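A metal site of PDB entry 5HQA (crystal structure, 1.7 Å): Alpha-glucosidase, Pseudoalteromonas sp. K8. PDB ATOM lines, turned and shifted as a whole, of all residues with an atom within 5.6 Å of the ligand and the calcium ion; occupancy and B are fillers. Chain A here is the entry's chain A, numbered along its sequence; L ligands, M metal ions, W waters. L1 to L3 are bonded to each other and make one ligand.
O6 of LG3 L3 is in hydrogen-bond range of NE1 of Trp 270 (3.0 Å). The side-chain amino group of Lys 386 sits at hydrogen-bond distance from an oxygen (O5) of LG3 L3 (2.8 Å). OE1 of Glu 358 sits at hydrogen-bond distance from O7 of LG3 L3 (2.9 Å). NH2 of Arg 152 is in hydrogen-bond range of O1 of LG3 L3, at 3.3 Å. An oxygen (O4) of LG3 L3 sits close to a ring nitrogen (ND1) of His 436. The side-chain amide oxygen (OD1) of Asn 151 lies within hydrogen-bond range of an oxygen (O1) of LG3 L3 (3.5 Å). An oxygen (O6) of LG3 L3 lies within hydrogen-bond range of the side-chain carboxylate (OE1) of Glu 311 (2.6 Å). O of Trp 465 lies within hydrogen-bond range of O3 of LIG L1, 3.4 Å away. NE2 of His 356 lies close to O7 of LG3 L3 (3.2 Å). An oxygen (O1) of LIG L1 sits at hydrogen-bond distance from the backbone carbonyl oxygen (O) of Thr 467 (3.5 Å). A ring nitrogen (NE2) of His 274 is in hydrogen-bond range of an oxygen (O6) of LG3 L3, 2.9 Å away.
OE2 of Glu 311 is in salt-bridge range of NZ of Lys 386 (2.7 Å). OE1 of Glu 311 is in hydrogen-bond range of NE1 of Trp 280. The indole nitrogen of Trp 270 sits at hydrogen-bond distance from a ring nitrogen (NE2) of His 274 (3.3 Å). ND1 of His 274 is in hydrogen-bond range of NE1 of Trp 465, at 2.9 Å. The backbone carbonyl oxygen (O) of Trp 465 is in hydrogen-bond range of the side-chain hydroxyl (OG1) of Thr 467, 2.8 Å away. OE2 of Glu 311 is in hydrogen-bond range of NE2 of His 356 (3.3 Å). OE2 of Glu 154 is in salt-bridge range of NH2 of Arg 152 (2.6 Å). The backbone carbonyl oxygen (O) of Glu 461 sits close to the indole nitrogen (NE1) of Trp 465.
Merely in contact with the ligand: Gly 466, Val 390, Trp 317, Trp 280, Trp 321 and Phe 462. Hydrophobic or aromatic side chains that line the ligand: Trp 270, His 274, Trp 280, Trp 317, Trp 321, His 356, Val 390, His 436, Phe 462 and Trp 465. Of the 27 residues printed, 21 come within 4 Å of the ligand. Along chain A the residues within 4 Å of the ligand span positions 151 to 467.
The calcium ion is bound by OE1 of Glu 455, OE2 of Glu 461, O2 of LG3 L3, O4 of LG3 L3, OE2 of Glu 437, OE1 of Glu 154 and N1 of LG3 L3.
Water W1 lies within hydrogen-bond range of the side-chain carboxylate of Glu 455, an oxygen (O5) of LG3 L3 and the side-chain carboxylate of Glu 461. Water W7 bridges O6 of LIG L1 (2.8 Å) and OD1 of Asn 151 (3.1 Å). Water W6 bridges OE1 of Glu 358 (2.5 Å) and OE1 of Glu 437 (2.5 Å).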
ATOM      1  N   TRP A 150      33.038   7.090  36.893  1.00  0.00           N
ATOM      2  CA  TRP A 150      31.760   7.565  36.373  1.00  0.00           C
ATOM      3  C   TRP A 150      31.930   8.734  35.414  1.00  0.00           C
ATOM      4  O   TRP A 150      31.052   8.962  34.563  1.00  0.00           O
ATOM      5  CB  TRP A 150      30.824   7.971  37.517  1.00  0.00           C
ATOM      6  CG  TRP A 150      31.214   9.239  38.182  1.00  0.00           C
ATOM      7  CD1 TRP A 150      32.112   9.402  39.204  1.00  0.00           C
ATOM      8  CD2 TRP A 150      30.712  10.557  37.883  1.00  0.00           C
ATOM      9  NE1 TRP A 150      32.207  10.729  39.544  1.00  0.00           N
ATOM     10  CE2 TRP A 150      31.361  11.458  38.753  1.00  0.00           C
ATOM     11  CE3 TRP A 150      29.789  11.044  36.966  1.00  0.00           C
ATOM     12  CZ2 TRP A 150      31.104  12.813  38.728  1.00  0.00           C
ATOM     13  CZ3 TRP A 150      29.537  12.406  36.946  1.00  0.00           C
ATOM     14  CH2 TRP A 150      30.204  13.279  37.816  1.00  0.00           C
ATOM     15  N   ASN A 151      33.052   9.468  35.493  1.00  0.00           N
ATOM     16  CA  ASN A 151      33.239  10.634  34.625  1.00  0.00           C
ATOM     17  C   ASN A 151      34.227  10.407  33.495  1.00  0.00           C
ATOM     18  O   ASN A 151      34.748  11.388  32.943  1.00  0.00           O
ATOM     19  CB  ASN A 151      33.646  11.874  35.440  1.00  0.00           C
ATOM     20  CG  ASN A 151      32.914  13.128  34.969  1.00  0.00           C
ATOM     21  OD1 ASN A 151      31.751  13.051  34.567  1.00  0.00           O
ATOM     22  ND2 ASN A 151      33.589  14.267  34.993  1.00  0.00           N
ATOM     23  N   ARG A 152      34.497   9.160  33.108  1.00  0.00           N
ATOM     24  CA  ARG A 152      35.189   8.833  31.845  1.00  0.00           C
ATOM     25  C   ARG A 152      36.615   9.412  31.899  1.00  0.00           C
ATOM     26  O   ARG A 152      37.365   9.100  32.838  1.00  0.00           O
ATOM     27  CB  ARG A 152      34.354   9.323  30.659  1.00  0.00           C
ATOM     28  CG  ARG A 152      32.903   8.781  30.584  1.00  0.00           C
ATOM     29  CD  ARG A 152      32.119   9.531  29.490  1.00  0.00           C
ATOM     30  NE  ARG A 152      32.405  10.947  29.605  1.00  0.00           N
ATOM     31  CZ  ARG A 152      31.747  11.786  30.397  1.00  0.00           C
ATOM     32  NH1 ARG A 152      30.721  11.357  31.110  1.00  0.00           N
ATOM     33  NH2 ARG A 152      32.123  13.048  30.463  1.00  0.00           N
ATOM     34  N   GLU A 154      37.199  12.683  32.103  1.00  0.00           N
ATOM     35  CA  GLU A 154      37.110  14.056  32.598  1.00  0.00           C
ATOM     36  C   GLU A 154      37.388  14.092  34.112  1.00  0.00           C
ATOM     37  O   GLU A 154      36.505  14.240  34.949  1.00  0.00           O
ATOM     38  CB  GLU A 154      35.741  14.648  32.251  1.00  0.00           C
ATOM     39  CG  GLU A 154      35.608  14.959  30.746  1.00  0.00           C
ATOM     40  CD  GLU A 154      34.212  15.454  30.361  1.00  0.00           C
ATOM     41  OE1 GLU A 154      34.076  16.034  29.263  1.00  0.00           O
ATOM     42  OE2 GLU A 154      33.259  15.250  31.138  1.00  0.00           O
ATOM     43  N   TRP A 270      27.262  28.804  23.011  1.00  0.00           N
ATOM     44  CA  TRP A 270      27.848  27.701  23.759  1.00  0.00           C
ATOM     45  C   TRP A 270      28.090  28.085  25.219  1.00  0.00           C
ATOM     46  O   TRP A 270      27.406  27.577  26.109  1.00  0.00           O
ATOM     47  CB  TRP A 270      29.159  27.253  23.092  1.00  0.00           C
ATOM     48  CG  TRP A 270      29.781  26.130  23.852  1.00  0.00           C
ATOM     49  CD1 TRP A 270      29.345  24.833  23.905  1.00  0.00           C
ATOM     50  CD2 TRP A 270      30.938  26.199  24.699  1.00  0.00           C
ATOM     51  NE1 TRP A 270      30.152  24.093  24.737  1.00  0.00           N
ATOM     52  CE2 TRP A 270      31.136  24.914  25.242  1.00  0.00           C
ATOM     53  CE3 TRP A 270      31.818  27.229  25.071  1.00  0.00           C
ATOM     54  CZ2 TRP A 270      32.175  24.618  26.128  1.00  0.00           C
ATOM     55  CZ3 TRP A 270      32.847  26.938  25.944  1.00  0.00           C
ATOM     56  CH2 TRP A 270      33.017  25.648  26.461  1.00  0.00           C
ATOM     57  N   HIS A 274      26.581  27.316  29.364  1.00  0.00           N
ATOM     58  CA  HIS A 274      27.365  26.807  30.494  1.00  0.00           C
ATOM     59  C   HIS A 274      27.363  27.762  31.680  1.00  0.00           C
ATOM     60  O   HIS A 274      27.449  27.304  32.831  1.00  0.00           O
ATOM     61  CB  HIS A 274      28.792  26.500  30.051  1.00  0.00           C
ATOM     62  CG  HIS A 274      28.885  25.245  29.259  1.00  0.00           C
ATOM     63  ND1 HIS A 274      29.036  24.011  29.846  1.00  0.00           N
ATOM     64  CD2 HIS A 274      28.773  25.019  27.926  1.00  0.00           C
ATOM     65  CE1 HIS A 274      29.045  23.076  28.915  1.00  0.00           C
ATOM     66  NE2 HIS A 274      28.887  23.666  27.741  1.00  0.00           N
ATOM     67  N   TRP A 280      19.780  25.506  26.515  1.00  0.00           N
ATOM     68  CA  TRP A 280      19.771  24.666  25.329  1.00  0.00           C
ATOM     69  C   TRP A 280      18.349  24.449  24.843  1.00  0.00           C
ATOM     70  O   TRP A 280      18.080  24.448  23.633  1.00  0.00           O
ATOM     71  CB  TRP A 280      20.417  23.317  25.618  1.00  0.00           C
ATOM     72  CG  TRP A 280      21.928  23.278  25.635  1.00  0.00           C
ATOM     73  CD1 TRP A 280      22.763  23.120  24.561  1.00  0.00           C
ATOM     74  CD2 TRP A 280      22.780  23.350  26.793  1.00  0.00           C
ATOM     75  NE1 TRP A 280      24.078  23.098  24.973  1.00  0.00           N
ATOM     76  CE2 TRP A 280      24.116  23.239  26.337  1.00  0.00           C
ATOM     77  CE3 TRP A 280      22.540  23.501  28.156  1.00  0.00           C
ATOM     78  CZ2 TRP A 280      25.215  23.272  27.202  1.00  0.00           C
ATOM     79  CZ3 TRP A 280      23.637  23.528  29.028  1.00  0.00           C
ATOM     80  CH2 TRP A 280      24.953  23.426  28.546  1.00  0.00           C
ATOM     81  N   GLU A 311      24.694  25.093  19.694  1.00  0.00           N
ATOM     82  CA  GLU A 311      24.122  23.971  20.407  1.00  0.00           C
ATOM     83  C   GLU A 311      22.697  24.282  20.843  1.00  0.00           C
ATOM     84  O   GLU A 311      22.373  25.429  21.180  1.00  0.00           O
ATOM     85  CB  GLU A 311      24.953  23.582  21.635  1.00  0.00           C
ATOM     86  CG  GLU A 311      26.379  23.225  21.282  1.00  0.00           C
ATOM     87  CD  GLU A 311      27.143  22.624  22.445  1.00  0.00           C
ATOM     88  OE1 GLU A 311      26.611  22.598  23.574  1.00  0.00           O
ATOM     89  OE2 GLU A 311      28.299  22.194  22.225  1.00  0.00           O
ATOM     90  N   TRP A 317      15.980  18.993  23.503  1.00  0.00           N
ATOM     91  CA  TRP A 317      16.699  19.537  24.645  1.00  0.00           C
ATOM     92  C   TRP A 317      15.778  19.966  25.785  1.00  0.00           C
ATOM     93  O   TRP A 317      16.274  20.213  26.888  1.00  0.00           O
ATOM     94  CB  TRP A 317      17.560  20.726  24.239  1.00  0.00           C
ATOM     95  CG  TRP A 317      18.717  20.383  23.326  1.00  0.00           C
ATOM     96  CD1 TRP A 317      18.673  20.287  21.966  1.00  0.00           C
ATOM     97  CD2 TRP A 317      20.064  20.093  23.707  1.00  0.00           C
ATOM     98  NE1 TRP A 317      19.909  19.964  21.469  1.00  0.00           N
ATOM     99  CE2 TRP A 317      20.790  19.832  22.512  1.00  0.00           C
ATOM    100  CE3 TRP A 317      20.739  20.025  24.935  1.00  0.00           C
ATOM    101  CZ2 TRP A 317      22.150  19.514  22.515  1.00  0.00           C
ATOM    102  CZ3 TRP A 317      22.108  19.702  24.937  1.00  0.00           C
ATOM    103  CH2 TRP A 317      22.791  19.449  23.733  1.00  0.00           C
ATOM    104  N   TRP A 321      18.087  17.681  29.554  1.00  0.00           N
ATOM    105  CA  TRP A 321      18.582  17.069  28.319  1.00  0.00           C
ATOM    106  C   TRP A 321      19.499  15.872  28.604  1.00  0.00           C
ATOM    107  O   TRP A 321      19.640  15.008  27.730  1.00  0.00           O
ATOM    108  CB  TRP A 321      19.301  18.104  27.459  1.00  0.00           C
ATOM    109  CG  TRP A 321      20.533  18.702  28.086  1.00  0.00           C
ATOM    110  CD1 TRP A 321      20.606  19.874  28.778  1.00  0.00           C
ATOM    111  CD2 TRP A 321      21.860  18.160  28.077  1.00  0.00           C
ATOM    112  NE1 TRP A 321      21.899  20.101  29.201  1.00  0.00           N
ATOM    113  CE2 TRP A 321      22.684  19.061  28.781  1.00  0.00           C
ATOM    114  CE3 TRP A 321      22.437  17.010  27.535  1.00  0.00           C
ATOM    115  CZ2 TRP A 321      24.050  18.845  28.967  1.00  0.00           C
ATOM    116  CZ3 TRP A 321      23.803  16.794  27.722  1.00  0.00           C
ATOM    117  CH2 TRP A 321      24.587  17.703  28.430  1.00  0.00           C
ATOM    118  N   PHE A 322      20.112  15.803  29.797  1.00  0.00           N
ATOM    119  CA  PHE A 322      20.938  14.639  30.148  1.00  0.00           C
ATOM    120  C   PHE A 322      20.144  13.338  30.025  1.00  0.00           C
ATOM    121  O   PHE A 322      20.744  12.281  29.781  1.00  0.00           O
ATOM    122  CB  PHE A 322      21.491  14.804  31.580  1.00  0.00           C
ATOM    123  CG  PHE A 322      22.369  13.654  32.059  1.00  0.00           C
ATOM    124  CD1 PHE A 322      21.828  12.551  32.709  1.00  0.00           C
ATOM    125  CD2 PHE A 322      23.757  13.703  31.905  1.00  0.00           C
ATOM    126  CE1 PHE A 322      22.628  11.504  33.168  1.00  0.00           C
ATOM    127  CE2 PHE A 322      24.565  12.651  32.363  1.00  0.00           C
ATOM    128  CZ  PHE A 322      24.004  11.557  32.987  1.00  0.00           C
ATOM    129  N   HIS A 356      26.026  20.285  15.333  1.00  0.00           N
ATOM    130  CA  HIS A 356      26.127  19.751  16.689  1.00  0.00           C
ATOM    131  C   HIS A 356      25.155  18.586  16.834  1.00  0.00           C
ATOM    132  O   HIS A 356      23.954  18.752  16.595  1.00  0.00           O
ATOM    133  CB  HIS A 356      25.817  20.814  17.740  1.00  0.00           C
ATOM    134  CG  HIS A 356      26.049  20.333  19.139  1.00  0.00           C
ATOM    135  ND1 HIS A 356      25.071  20.387  20.119  1.00  0.00           N
ATOM    136  CD2 HIS A 356      27.134  19.768  19.720  1.00  0.00           C
ATOM    137  CE1 HIS A 356      25.560  19.898  21.249  1.00  0.00           C
ATOM    138  NE2 HIS A 356      26.804  19.514  21.029  1.00  0.00           N
ATOM    139  N   GLU A 358      24.482  16.111  19.837  1.00  0.00           N
ATOM    140  CA  GLU A 358      24.570  15.522  21.163  1.00  0.00           C
ATOM    141  C   GLU A 358      23.633  14.326  21.250  1.00  0.00           C
ATOM    142  O   GLU A 358      22.448  14.432  20.914  1.00  0.00           O
ATOM    143  CB  GLU A 358      24.213  16.543  22.246  1.00  0.00           C
ATOM    144  CG  GLU A 358      24.144  15.938  23.658  1.00  0.00           C
ATOM    145  CD  GLU A 358      25.490  15.352  24.115  1.00  0.00           C
ATOM    146  OE1 GLU A 358      26.493  16.088  24.166  1.00  0.00           O
ATOM    147  OE2 GLU A 358      25.536  14.136  24.413  1.00  0.00           O
ATOM    148  N   LYS A 386      30.342  18.986  15.690  1.00  0.00           N
ATOM    149  CA  LYS A 386      30.723  18.581  17.028  1.00  0.00           C
ATOM    150  C   LYS A 386      29.730  17.515  17.497  1.00  0.00           C
ATOM    151  O   LYS A 386      28.518  17.767  17.488  1.00  0.00           O
ATOM    152  CB  LYS A 386      30.712  19.778  17.971  1.00  0.00           C
ATOM    153  CG  LYS A 386      30.979  19.461  19.431  1.00  0.00           C
ATOM    154  CD  LYS A 386      30.947  20.753  20.255  1.00  0.00           C
ATOM    155  CE  LYS A 386      31.064  20.456  21.739  1.00  0.00           C
ATOM    156  NZ  LYS A 386      30.917  21.701  22.517  1.00  0.00           N
ATOM    157  N   GLY A 388      28.623  14.503  20.565  1.00  0.00           N
ATOM    158  CA  GLY A 388      28.640  14.412  22.016  1.00  0.00           C
ATOM    159  C   GLY A 388      28.006  13.126  22.472  1.00  0.00           C
ATOM    160  O   GLY A 388      27.058  12.625  21.856  1.00  0.00           O
ATOM    161  N   VAL A 390      27.155  12.322  26.091  1.00  0.00           N
ATOM    162  CA  VAL A 390      27.102  12.574  27.536  1.00  0.00           C
ATOM    163  C   VAL A 390      26.320  11.440  28.220  1.00  0.00           C
ATOM    164  O   VAL A 390      25.106  11.295  28.030  1.00  0.00           O
ATOM    165  CB  VAL A 390      26.486  13.937  27.857  1.00  0.00           C
ATOM    166  CG1 VAL A 390      26.308  14.093  29.369  1.00  0.00           C
ATOM    167  CG2 VAL A 390      27.386  15.033  27.325  1.00  0.00           C
ATOM    168  N   ASP A 392      27.205   8.667  31.984  1.00  0.00           N
ATOM    169  CA  ASP A 392      28.205   8.205  32.933  1.00  0.00           C
ATOM    170  C   ASP A 392      29.007   7.043  32.335  1.00  0.00           C
ATOM    171  O   ASP A 392      28.563   6.366  31.398  1.00  0.00           O
ATOM    172  CB  ASP A 392      27.568   7.761  34.233  1.00  0.00           C
ATOM    173  CG  ASP A 392      27.081   8.925  35.091  1.00  0.00           C
ATOM    174  OD1 ASP A 392      27.200  10.100  34.646  1.00  0.00           O
ATOM    175  OD2 ASP A 392      26.582   8.650  36.202  1.00  0.00           O
ATOM    176  N   HIS A 436      33.202  15.074  21.373  1.00  0.00           N
ATOM    177  CA  HIS A 436      33.220  15.193  22.827  1.00  0.00           C
ATOM    178  C   HIS A 436      32.705  13.905  23.461  1.00  0.00           C
ATOM    179  O   HIS A 436      31.909  13.172  22.867  1.00  0.00           O
ATOM    180  CB  HIS A 436      32.422  16.415  23.290  1.00  0.00           C
ATOM    181  CG  HIS A 436      33.158  17.703  23.071  1.00  0.00           C
ATOM    182  ND1 HIS A 436      33.207  18.712  24.009  1.00  0.00           N
ATOM    183  CD2 HIS A 436      33.904  18.121  22.017  1.00  0.00           C
ATOM    184  CE1 HIS A 436      33.944  19.709  23.543  1.00  0.00           C
ATOM    185  NE2 HIS A 436      34.376  19.374  22.336  1.00  0.00           N
ATOM    186  N   GLU A 437      33.177  13.643  24.689  1.00  0.00           N
ATOM    187  CA  GLU A 437      33.071  12.332  25.323  1.00  0.00           C
ATOM    188  C   GLU A 437      33.485  11.239  24.325  1.00  0.00           C
ATOM    189  O   GLU A 437      32.684  10.373  23.966  1.00  0.00           O
ATOM    190  CB  GLU A 437      31.672  12.062  25.876  1.00  0.00           C
ATOM    191  CG  GLU A 437      31.253  13.105  26.914  1.00  0.00           C
ATOM    192  CD  GLU A 437      30.873  14.433  26.263  1.00  0.00           C
ATOM    193  OE1 GLU A 437      30.094  14.398  25.293  1.00  0.00           O
ATOM    194  OE2 GLU A 437      31.391  15.500  26.685  1.00  0.00           O
ATOM    195  N   GLU A 455      37.550  16.028  22.686  1.00  0.00           N
ATOM    196  CA  GLU A 455      37.730  16.493  24.054  1.00  0.00           C
ATOM    197  C   GLU A 455      38.458  15.403  24.847  1.00  0.00           C
ATOM    198  O   GLU A 455      39.679  15.290  24.764  1.00  0.00           O
ATOM    199  CB  GLU A 455      36.376  16.880  24.653  1.00  0.00           C
ATOM    200  CG  GLU A 455      36.472  17.676  25.939  1.00  0.00           C
ATOM    201  CD  GLU A 455      35.112  18.102  26.449  1.00  0.00           C
ATOM    202  OE1 GLU A 455      34.262  17.215  26.699  1.00  0.00           O
ATOM    203  OE2 GLU A 455      34.876  19.320  26.576  1.00  0.00           O
ATOM    204  N   ARG A 458      39.182  17.080  30.950  1.00  0.00           N
ATOM    205  CA  ARG A 458      38.515  18.284  31.434  1.00  0.00           C
ATOM    206  C   ARG A 458      39.017  19.508  30.664  1.00  0.00           C
ATOM    207  O   ARG A 458      40.205  19.838  30.719  1.00  0.00           O
ATOM    208  CB  ARG A 458      38.750  18.461  32.927  1.00  0.00           C
ATOM    209  CG  ARG A 458      37.903  17.527  33.774  1.00  0.00           C
ATOM    210  CD  ARG A 458      38.252  17.642  35.265  1.00  0.00           C
ATOM    211  NE  ARG A 458      38.088  19.004  35.778  1.00  0.00           N
ATOM    212  CZ  ARG A 458      37.381  19.329  36.871  1.00  0.00           C
ATOM    213  NH1 ARG A 458      36.755  18.388  37.576  1.00  0.00           N
ATOM    214  NH2 ARG A 458      37.312  20.595  37.251  1.00  0.00           N
ATOM    215  N   GLU A 461      34.956  23.978  29.953  1.00  0.00           N
ATOM    216  CA  GLU A 461      33.597  23.907  30.492  1.00  0.00           C
ATOM    217  C   GLU A 461      33.590  23.638  31.989  1.00  0.00           C
ATOM    218  O   GLU A 461      32.707  24.142  32.704  1.00  0.00           O
ATOM    219  CB  GLU A 461      32.797  22.821  29.771  1.00  0.00           C
ATOM    220  CG  GLU A 461      33.428  21.433  29.866  1.00  0.00           C
ATOM    221  CD  GLU A 461      32.533  20.346  29.287  1.00  0.00           C
ATOM    222  OE1 GLU A 461      31.359  20.659  28.982  1.00  0.00           O
ATOM    223  OE2 GLU A 461      32.999  19.195  29.146  1.00  0.00           O
ATOM    224  N   PHE A 462      34.554  22.868  32.504  1.00  0.00           N
ATOM    225  CA  PHE A 462      34.584  22.626  33.944  1.00  0.00           C
ATOM    226  C   PHE A 462      34.913  23.876  34.740  1.00  0.00           C
ATOM    227  O   PHE A 462      34.717  23.869  35.960  1.00  0.00           O
ATOM    228  CB  PHE A 462      35.578  21.508  34.284  1.00  0.00           C
ATOM    229  CG  PHE A 462      35.019  20.144  34.036  1.00  0.00           C
ATOM    230  CD1 PHE A 462      35.014  19.610  32.744  1.00  0.00           C
ATOM    231  CD2 PHE A 462      34.462  19.406  35.065  1.00  0.00           C
ATOM    232  CE1 PHE A 462      34.466  18.357  32.499  1.00  0.00           C
ATOM    233  CE2 PHE A 462      33.915  18.155  34.834  1.00  0.00           C
ATOM    234  CZ  PHE A 462      33.915  17.627  33.548  1.00  0.00           C
ATOM    235  N   TRP A 465      31.345  25.432  35.931  1.00  0.00           N
ATOM    236  CA  TRP A 465      30.502  24.824  36.950  1.00  0.00           C
ATOM    237  C   TRP A 465      31.175  23.669  37.706  1.00  0.00           C
ATOM    238  O   TRP A 465      30.474  22.963  38.443  1.00  0.00           O
ATOM    239  CB  TRP A 465      29.185  24.319  36.318  1.00  0.00           C
ATOM    240  CG  TRP A 465      29.402  23.735  34.931  1.00  0.00           C
ATOM    241  CD1 TRP A 465      29.044  24.310  33.740  1.00  0.00           C
ATOM    242  CD2 TRP A 465      30.046  22.495  34.603  1.00  0.00           C
ATOM    243  NE1 TRP A 465      29.405  23.500  32.689  1.00  0.00           N
ATOM    244  CE2 TRP A 465      30.025  22.386  33.191  1.00  0.00           C
ATOM    245  CE3 TRP A 465      30.623  21.472  35.353  1.00  0.00           C
ATOM    246  CZ2 TRP A 465      30.574  21.281  32.521  1.00  0.00           C
ATOM    247  CZ3 TRP A 465      31.166  20.374  34.697  1.00  0.00           C
ATOM    248  CH2 TRP A 465      31.140  20.294  33.291  1.00  0.00           C
ATOM    249  N   GLY A 466      32.493  23.454  37.562  1.00  0.00           N
ATOM    250  CA  GLY A 466      33.081  22.185  37.974  1.00  0.00           C
ATOM    251  C   GLY A 466      32.922  21.882  39.459  1.00  0.00           C
ATOM    252  O   GLY A 466      32.720  20.713  39.842  1.00  0.00           O
ATOM    253  N   THR A 467      33.002  22.915  40.297  1.00  0.00           N
ATOM    254  CA  THR A 467      32.824  22.775  41.749  1.00  0.00           C
ATOM    255  C   THR A 467      33.658  21.632  42.355  1.00  0.00           C
ATOM    256  O   THR A 467      33.089  20.669  42.889  1.00  0.00           O
ATOM    257  CB  THR A 467      31.325  22.559  42.103  1.00  0.00           C
ATOM    258  OG1 THR A 467      30.510  23.365  41.238  1.00  0.00           O
ATOM    259  CG2 THR A 467      31.048  22.985  43.526  1.00  0.00           C
ATOM    260  N   PRO A 468      34.995  21.738  42.310  1.00  0.00           N
ATOM    261  CA  PRO A 468      35.780  22.886  41.875  1.00  0.00           C
ATOM    262  C   PRO A 468      36.091  22.921  40.386  1.00  0.00           C
ATOM    263  O   PRO A 468      36.009  21.887  39.684  1.00  0.00           O
ATOM    264  CB  PRO A 468      37.090  22.712  42.673  1.00  0.00           C
ATOM    265  CG  PRO A 468      37.261  21.236  42.712  1.00  0.00           C
ATOM    266  CD  PRO A 468      35.847  20.700  42.918  1.00  0.00           C
HETATM  267  C1  LIG L   1      29.964  19.128  40.746  1.00  0.00           C
HETATM  268  C2  LIG L   1      28.660  19.896  40.591  1.00  0.00           C
HETATM  269  C3  LIG L   1      27.905  19.711  39.302  1.00  0.00           C
HETATM  270  C4  LIG L   1      28.459  18.793  38.257  1.00  0.00           C
HETATM  271  C5  LIG L   1      29.644  17.900  38.639  1.00  0.00           C
HETATM  272  C6  LIG L   1      30.893  18.287  37.937  1.00  0.00           C
HETATM  273  O1  LIG L   1      30.222  18.924  42.090  1.00  0.00           O
HETATM  274  O2  LIG L   1      27.768  19.527  41.653  1.00  0.00           O
HETATM  275  O3  LIG L   1      27.687  21.044  38.722  1.00  0.00           O
HETATM  276  O4  LIG L   1      27.383  17.800  37.943  1.00  0.00           O
HETATM  277  O5  LIG L   1      29.906  17.803  40.094  1.00  0.00           O
HETATM  278  O6  LIG L   1      31.522  17.088  37.544  1.00  0.00           O
HETATM  279  C1  LG2 L   2      26.581  18.067  36.843  1.00  0.00           C
HETATM  280  C2  LG2 L   2      26.349  16.758  36.105  1.00  0.00           C
HETATM  281  C3  LG2 L   2      27.494  16.374  35.210  1.00  0.00           C
HETATM  282  C4  LG2 L   2      27.671  17.415  34.154  1.00  0.00           C
HETATM  283  C5  LG2 L   2      27.899  18.811  34.750  1.00  0.00           C
HETATM  284  C6  LG2 L   2      27.559  19.852  33.718  1.00  0.00           C
HETATM  285  O1  LG2 L   2      26.124  15.726  37.087  1.00  0.00           O
HETATM  286  O2  LG2 L   2      27.212  15.066  34.593  1.00  0.00           O
HETATM  287  O3  LG2 L   2      28.807  17.058  33.237  1.00  0.00           O
HETATM  288  O4  LG2 L   2      27.109  19.175  35.980  1.00  0.00           O
HETATM  289  O5  LG2 L   2      26.180  20.139  33.713  1.00  0.00           O
HETATM  290  C1  LG3 L   3      28.309  16.493  32.069  1.00  0.00           C
HETATM  291  O1  LG3 L   3      30.252  15.108  32.166  1.00  0.00           O
HETATM  292  C2  LG3 L   3      29.403  15.827  31.255  1.00  0.00           C
HETATM  293  C3  LG3 L   3      28.616  20.590  25.405  1.00  0.00           C
HETATM  294  C4  LG3 L   3      30.189  16.830  30.446  1.00  0.00           C
HETATM  295  O2  LG3 L   3      31.265  16.178  29.748  1.00  0.00           O
HETATM  296  C5  LG3 L   3      29.262  17.541  29.503  1.00  0.00           C
HETATM  297  N1  LG3 L   3      29.978  18.347  28.462  1.00  0.00           N
HETATM  298  C6  LG3 L   3      28.481  18.426  30.472  1.00  0.00           C
HETATM  299  O3  LG3 L   3      27.591  17.542  31.263  1.00  0.00           O
HETATM  300  C7  LG3 L   3      27.650  19.485  29.823  1.00  0.00           C
HETATM  301  C8  LG3 L   3      29.501  18.130  27.047  1.00  0.00           C
HETATM  302  C9  LG3 L   3      30.437  19.007  25.979  1.00  0.00           C
HETATM  303  O4  LG3 L   3      31.793  18.724  26.279  1.00  0.00           O
HETATM  304  C10 LG3 L   3      30.110  20.375  26.025  1.00  0.00           C
HETATM  305  O5  LG3 L   3      31.023  21.198  25.251  1.00  0.00           O
HETATM  306  O6  LG3 L   3      28.211  21.932  25.557  1.00  0.00           O
HETATM  307  C11 LG3 L   3      27.629  19.725  25.999  1.00  0.00           C
HETATM  308  C12 LG3 L   3      28.120  18.419  26.842  1.00  0.00           C
HETATM  309  C13 LG3 L   3      26.232  19.701  25.351  1.00  0.00           C
HETATM  310  O7  LG3 L   3      26.336  18.990  24.153  1.00  0.00           O
HETATM  311 CA    CA M   1      32.380  17.273  28.023  1.00  0.00          CA
HETATM  312  O   HOH W   1      33.379  21.440  26.352  1.00  0.00           O
HETATM  313  O   HOH W   2      33.556  15.677  38.433  1.00  0.00           O
HETATM  314  O   HOH W   3      30.396  15.520  41.142  1.00  0.00           O
HETATM  315  O   HOH W   4      31.649  16.148  43.668  1.00  0.00           O
HETATM  316  O   HOH W   5      23.282  14.781  35.809  1.00  0.00           O
HETATM  317  O   HOH W   6      28.939  16.509  24.503  1.00  0.00           O
HETATM  318  O   HOH W   7      30.642  15.947  35.114  1.00  0.00           O
